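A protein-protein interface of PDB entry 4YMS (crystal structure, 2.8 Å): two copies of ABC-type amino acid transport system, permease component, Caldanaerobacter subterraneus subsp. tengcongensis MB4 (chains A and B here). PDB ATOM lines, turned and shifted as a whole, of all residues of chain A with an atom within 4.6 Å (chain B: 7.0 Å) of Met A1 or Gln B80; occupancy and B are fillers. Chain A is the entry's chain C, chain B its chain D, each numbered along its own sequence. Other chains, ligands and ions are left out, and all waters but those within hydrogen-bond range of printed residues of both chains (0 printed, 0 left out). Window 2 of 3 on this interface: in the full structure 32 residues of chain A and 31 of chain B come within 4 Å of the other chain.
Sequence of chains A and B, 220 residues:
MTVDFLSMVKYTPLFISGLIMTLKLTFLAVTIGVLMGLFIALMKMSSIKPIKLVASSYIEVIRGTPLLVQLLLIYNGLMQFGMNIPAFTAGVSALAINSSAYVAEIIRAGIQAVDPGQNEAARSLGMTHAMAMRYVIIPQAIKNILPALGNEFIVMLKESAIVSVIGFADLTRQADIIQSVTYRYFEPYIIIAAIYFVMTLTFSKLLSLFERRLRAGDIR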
ATOM      1  N   MET A   1      -4.415  18.128  30.551  1.00  0.00           N
ATOM      2  CA  MET A   1      -4.224  16.706  30.818  1.00  0.00           C
ATOM      3  C   MET A   1      -5.031  15.818  29.869  1.00  0.00           C
ATOM      4  O   MET A   1      -4.661  15.613  28.706  1.00  0.00           O
ATOM      5  CB  MET A   1      -4.604  16.376  32.257  1.00  0.00           C
ATOM      6  CG  MET A   1      -3.952  15.100  32.774  1.00  0.00           C
ATOM      7  SD  MET A   1      -4.713  14.571  34.315  1.00  0.00           S
ATOM      8  CE  MET A   1      -4.816  16.136  35.198  1.00  0.00           C
ATOM      9  N   THR A   2      -6.108  15.249  30.405  1.00  0.00           N
ATOM     10  CA  THR A   2      -7.130  14.582  29.602  1.00  0.00           C
ATOM     11  C   THR A   2      -8.495  15.120  30.052  1.00  0.00           C
ATOM     12  O   THR A   2      -8.585  15.855  31.041  1.00  0.00           O
ATOM     13  CB  THR A   2      -7.094  13.039  29.726  1.00  0.00           C
ATOM     14  OG1 THR A   2      -6.983  12.652  31.100  1.00  0.00           O
ATOM     15  CG2 THR A   2      -5.944  12.463  28.919  1.00  0.00           C
ATOM     16  N   TYR A 183      -6.744  25.702  33.188  1.00  0.00           N
ATOM     17  CA  TYR A 183      -5.831  25.306  32.107  1.00  0.00           C
ATOM     18  C   TYR A 183      -6.517  24.409  31.050  1.00  0.00           C
ATOM     19  O   TYR A 183      -5.860  23.835  30.174  1.00  0.00           O
ATOM     20  CB  TYR A 183      -4.574  24.630  32.711  1.00  0.00           C
ATOM     21  CG  TYR A 183      -3.943  25.496  33.805  1.00  0.00           C
ATOM     22  CD1 TYR A 183      -3.000  26.472  33.498  1.00  0.00           C
ATOM     23  CD2 TYR A 183      -4.339  25.368  35.134  1.00  0.00           C
ATOM     24  CE1 TYR A 183      -2.469  27.284  34.484  1.00  0.00           C
ATOM     25  CE2 TYR A 183      -3.819  26.170  36.119  1.00  0.00           C
ATOM     26  CZ  TYR A 183      -2.884  27.128  35.796  1.00  0.00           C
ATOM     27  OH  TYR A 183      -2.363  27.922  36.799  1.00  0.00           O
ATOM     28  N   ARG A 184      -7.851  24.369  31.092  1.00  0.00           N
ATOM     29  CA  ARG A 184      -8.649  23.588  30.133  1.00  0.00           C
ATOM     30  C   ARG A 184      -9.388  24.489  29.134  1.00  0.00           C
ATOM     31  O   ARG A 184     -10.141  25.383  29.523  1.00  0.00           O
ATOM     32  CB  ARG A 184      -9.653  22.692  30.877  1.00  0.00           C
ATOM     33  CG  ARG A 184      -8.982  21.647  31.751  1.00  0.00           C
ATOM     34  CD  ARG A 184      -9.949  20.703  32.457  1.00  0.00           C
ATOM     35  NE  ARG A 184      -9.213  19.642  33.147  1.00  0.00           N
ATOM     36  CZ  ARG A 184      -8.667  18.585  32.546  1.00  0.00           C
ATOM     37  NH1 ARG A 184      -8.785  18.423  31.232  1.00  0.00           N
ATOM     38  NH2 ARG A 184      -8.002  17.677  33.256  1.00  0.00           N
ATOM     39  N   TYR A 185      -9.149  24.254  27.842  1.00  0.00           N
ATOM     40  CA  TYR A 185      -9.805  25.016  26.772  1.00  0.00           C
ATOM     41  C   TYR A 185     -10.925  24.225  26.098  1.00  0.00           C
ATOM     42  O   TYR A 185     -12.011  24.736  25.889  1.00  0.00           O
ATOM     43  CB  TYR A 185      -8.774  25.451  25.727  1.00  0.00           C
ATOM     44  CG  TYR A 185      -8.278  26.865  25.903  1.00  0.00           C
ATOM     45  CD1 TYR A 185      -9.171  27.892  26.126  1.00  0.00           C
ATOM     46  CD2 TYR A 185      -6.921  27.179  25.817  1.00  0.00           C
ATOM     47  CE1 TYR A 185      -8.739  29.199  26.267  1.00  0.00           C
ATOM     48  CE2 TYR A 185      -6.474  28.487  25.956  1.00  0.00           C
ATOM     49  CZ  TYR A 185      -7.392  29.493  26.182  1.00  0.00           C
ATOM     50  OH  TYR A 185      -6.999  30.809  26.323  1.00  0.00           O
ATOM     51  N   PHE A 186     -10.633  22.973  25.769  1.00  0.00           N
ATOM     52  CA  PHE A 186     -11.571  22.055  25.144  1.00  0.00           C
ATOM     53  C   PHE A 186     -12.928  22.014  25.831  1.00  0.00           C
ATOM     54  O   PHE A 186     -13.927  22.454  25.264  1.00  0.00           O
ATOM     55  CB  PHE A 186     -10.956  20.665  25.137  1.00  0.00           C
ATOM     56  CG  PHE A 186     -11.760  19.631  24.415  1.00  0.00           C
ATOM     57  CD1 PHE A 186     -11.588  19.430  23.057  1.00  0.00           C
ATOM     58  CD2 PHE A 186     -12.652  18.822  25.105  1.00  0.00           C
ATOM     59  CE1 PHE A 186     -12.308  18.450  22.393  1.00  0.00           C
ATOM     60  CE2 PHE A 186     -13.380  17.836  24.449  1.00  0.00           C
ATOM     61  CZ  PHE A 186     -13.207  17.649  23.092  1.00  0.00           C
ATOM     62  N   GLU A 187     -12.963  21.488  27.050  1.00  0.00           N
ATOM     63  CA  GLU A 187     -14.235  21.265  27.738  1.00  0.00           C
ATOM     64  C   GLU A 187     -15.127  22.524  27.859  1.00  0.00           C
ATOM     65  O   GLU A 187     -16.324  22.450  27.572  1.00  0.00           O
ATOM     66  CB  GLU A 187     -14.006  20.656  29.133  1.00  0.00           C
ATOM     67  CG  GLU A 187     -12.595  20.793  29.717  1.00  0.00           C
ATOM     68  CD  GLU A 187     -11.657  19.623  29.430  1.00  0.00           C
ATOM     69  OE1 GLU A 187     -10.583  19.862  28.833  1.00  0.00           O
ATOM     70  OE2 GLU A 187     -11.944  18.488  29.874  1.00  0.00           O
ATOM     71  N   TYR B  75      -8.195  25.418  17.785  1.00  0.00           N
ATOM     72  CA  TYR B  75      -6.911  26.032  18.152  1.00  0.00           C
ATOM     73  C   TYR B  75      -6.562  25.857  19.630  1.00  0.00           C
ATOM     74  O   TYR B  75      -5.629  25.129  19.989  1.00  0.00           O
ATOM     75  CB  TYR B  75      -6.943  27.520  17.800  1.00  0.00           C
ATOM     76  CG  TYR B  75      -5.610  28.236  17.826  1.00  0.00           C
ATOM     77  CD1 TYR B  75      -5.366  29.268  18.738  1.00  0.00           C
ATOM     78  CD2 TYR B  75      -4.614  27.920  16.905  1.00  0.00           C
ATOM     79  CE1 TYR B  75      -4.156  29.957  18.746  1.00  0.00           C
ATOM     80  CE2 TYR B  75      -3.399  28.588  16.906  1.00  0.00           C
ATOM     81  CZ  TYR B  75      -3.174  29.609  17.828  1.00  0.00           C
ATOM     82  OH  TYR B  75      -1.963  30.272  17.828  1.00  0.00           O
ATOM     83  N   ASN B  76      -7.321  26.538  20.477  1.00  0.00           N
ATOM     84  CA  ASN B  76      -7.102  26.484  21.905  1.00  0.00           C
ATOM     85  C   ASN B  76      -7.430  25.123  22.495  1.00  0.00           C
ATOM     86  O   ASN B  76      -6.626  24.545  23.222  1.00  0.00           O
ATOM     87  CB  ASN B  76      -7.933  27.559  22.596  1.00  0.00           C
ATOM     88  CG  ASN B  76      -7.489  28.961  22.229  1.00  0.00           C
ATOM     89  OD1 ASN B  76      -6.435  29.152  21.618  1.00  0.00           O
ATOM     90  ND2 ASN B  76      -8.299  29.954  22.588  1.00  0.00           N
ATOM     91  N   GLY B  77      -8.583  24.582  22.141  1.00  0.00           N
ATOM     92  CA  GLY B  77      -9.042  23.364  22.767  1.00  0.00           C
ATOM     93  C   GLY B  77      -8.113  22.181  22.572  1.00  0.00           C
ATOM     94  O   GLY B  77      -8.152  21.234  23.358  1.00  0.00           O
ATOM     95  N   LEU B  78      -7.245  22.228  21.566  1.00  0.00           N
ATOM     96  CA  LEU B  78      -6.402  21.060  21.301  1.00  0.00           C
ATOM     97  C   LEU B  78      -5.045  21.116  21.979  1.00  0.00           C
ATOM     98  O   LEU B  78      -4.359  20.100  22.087  1.00  0.00           O
ATOM     99  CB  LEU B  78      -6.204  20.869  19.799  1.00  0.00           C
ATOM    100  CG  LEU B  78      -7.418  20.314  19.060  1.00  0.00           C
ATOM    101  CD1 LEU B  78      -6.990  19.820  17.696  1.00  0.00           C
ATOM    102  CD2 LEU B  78      -8.086  19.210  19.858  1.00  0.00           C
ATOM    103  N   MET B  79      -4.672  22.301  22.445  1.00  0.00           N
ATOM    104  CA  MET B  79      -3.390  22.515  23.105  1.00  0.00           C
ATOM    105  C   MET B  79      -3.181  21.544  24.249  1.00  0.00           C
ATOM    106  O   MET B  79      -2.152  20.864  24.325  1.00  0.00           O
ATOM    107  CB  MET B  79      -3.316  23.946  23.603  1.00  0.00           C
ATOM    108  CG  MET B  79      -2.876  24.893  22.526  1.00  0.00           C
ATOM    109  SD  MET B  79      -3.268  26.591  22.951  1.00  0.00           S
ATOM    110  CE  MET B  79      -2.695  27.430  21.473  1.00  0.00           C
ATOM    111  N   GLN B  80      -4.188  21.445  25.110  1.00  0.00           N
ATOM    112  CA  GLN B  80      -4.100  20.597  26.288  1.00  0.00           C
ATOM    113  C   GLN B  80      -3.912  19.117  25.969  1.00  0.00           C
ATOM    114  O   GLN B  80      -3.765  18.301  26.872  1.00  0.00           O
ATOM    115  CB  GLN B  80      -5.340  20.794  27.159  1.00  0.00           C
ATOM    116  CG  GLN B  80      -6.652  20.440  26.492  1.00  0.00           C
ATOM    117  CD  GLN B  80      -7.850  20.906  27.307  1.00  0.00           C
ATOM    118  OE1 GLN B  80      -8.226  22.086  27.278  1.00  0.00           O
ATOM    119  NE2 GLN B  80      -8.443  19.981  28.057  1.00  0.00           N
ATOM    120  N   PHE B  81      -3.921  18.768  24.687  1.00  0.00           N
ATOM    121  CA  PHE B  81      -3.631  17.402  24.266  1.00  0.00           C
ATOM    122  C   PHE B  81      -2.254  17.298  23.634  1.00  0.00           C
ATOM    123  O   PHE B  81      -1.946  16.328  22.945  1.00  0.00           O
ATOM    124  CB  PHE B  81      -4.686  16.922  23.284  1.00  0.00           C
ATOM    125  CG  PHE B  81      -6.070  16.989  23.826  1.00  0.00           C
ATOM    126  CD1 PHE B  81      -6.498  16.079  24.778  1.00  0.00           C
ATOM    127  CD2 PHE B  81      -6.950  17.966  23.390  1.00  0.00           C
ATOM    128  CE1 PHE B  81      -7.788  16.141  25.289  1.00  0.00           C
ATOM    129  CE2 PHE B  81      -8.240  18.031  23.891  1.00  0.00           C
ATOM    130  CZ  PHE B  81      -8.660  17.114  24.842  1.00  0.00           C
ATOM    131  N   GLY B  82      -1.427  18.305  23.881  1.00  0.00           N
ATOM    132  CA  GLY B  82      -0.094  18.352  23.311  1.00  0.00           C
ATOM    133  C   GLY B  82      -0.175  18.610  21.821  1.00  0.00           C
ATOM    134  O   GLY B  82       0.650  18.130  21.040  1.00  0.00           O
ATOM    135  N   MET B  83      -1.174  19.386  21.425  1.00  0.00           N
ATOM    136  CA  MET B  83      -1.368  19.687  20.021  1.00  0.00           C
ATOM    137  C   MET B  83      -1.092  21.152  19.786  1.00  0.00           C
ATOM    138  O   MET B  83      -1.625  22.024  20.479  1.00  0.00           O
ATOM    139  CB  MET B  83      -2.786  19.341  19.577  1.00  0.00           C
ATOM    140  CG  MET B  83      -3.181  17.898  19.798  1.00  0.00           C
ATOM    141  SD  MET B  83      -2.757  16.873  18.372  1.00  0.00           S
ATOM    142  CE  MET B  83      -3.782  17.628  17.102  1.00  0.00           C
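N of Tyr A185 sits at hydrogen-bond distance from OE1 of Gln B80.
The side-chain amide oxygen (OE1) of Gln B80 is in hydrogen-bond range of the backbone NH (N) of Phe A186 (3.0 Å).
O of Met A1 sits close to O of Gln B80.
OE1 of Glu A187 lies close to NE2 of Gln B80, 2.3 Å away.
The backbone carbonyl oxygen (O) of Thr A2 sits at hydrogen-bond distance from the guanidinium group (NH1) of Arg A184 (2.6 Å).
The guanidinium group of Arg A184 lies within salt-bridge range of the side-chain carboxylate of Glu A187 (3.3 Å).
Among the printed residues, pairs that only touch across the chains: Arg A184 with Gln B80, Phe A186 with Gly B77, Tyr A185 with Asn B76, Tyr A185 with Gly B77 and Phe A186 with Phe B81.
Of the printed residues of chain B, Arg A184 touches Gln B80.
Of the printed residues of chain B, Tyr A185 touches Asn B76 (3.4 Å), Gly B77 (3.6 Å) and Gln B80 (2.4 Å).
Of the printed residues of chain B, Phe A186 touches Gly B77, Gln B80 and Phe B81.
Printed residues of chain A within 4 Å of Phe B81: Phe A186 (3.7 Å).
Gly B82 touches none of the printed residues of chain A.
The nearest residue of chain B that does not touch Met A1 is Phe B81 (4.4 Å).
Hydrophobic or aromatic side chains of chain A that line the printed part of chain B: Tyr A185 and Phe A186.
Hydrophobic or aromatic side chains of chain B within 4 Å of the printed part of chain A: Phe B81.
Among the printed residues, 9 pairs touch across the chains.
Among the printed residues, no Asp or Glu carboxylate lies within 4 Å of a Lys or Arg side-chain nitrogen of the other chain.
No position is printed for both chains.
Of the 9 pairs that touch across the chains among the printed residues, none has its exchanged pair printed and touching as well.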
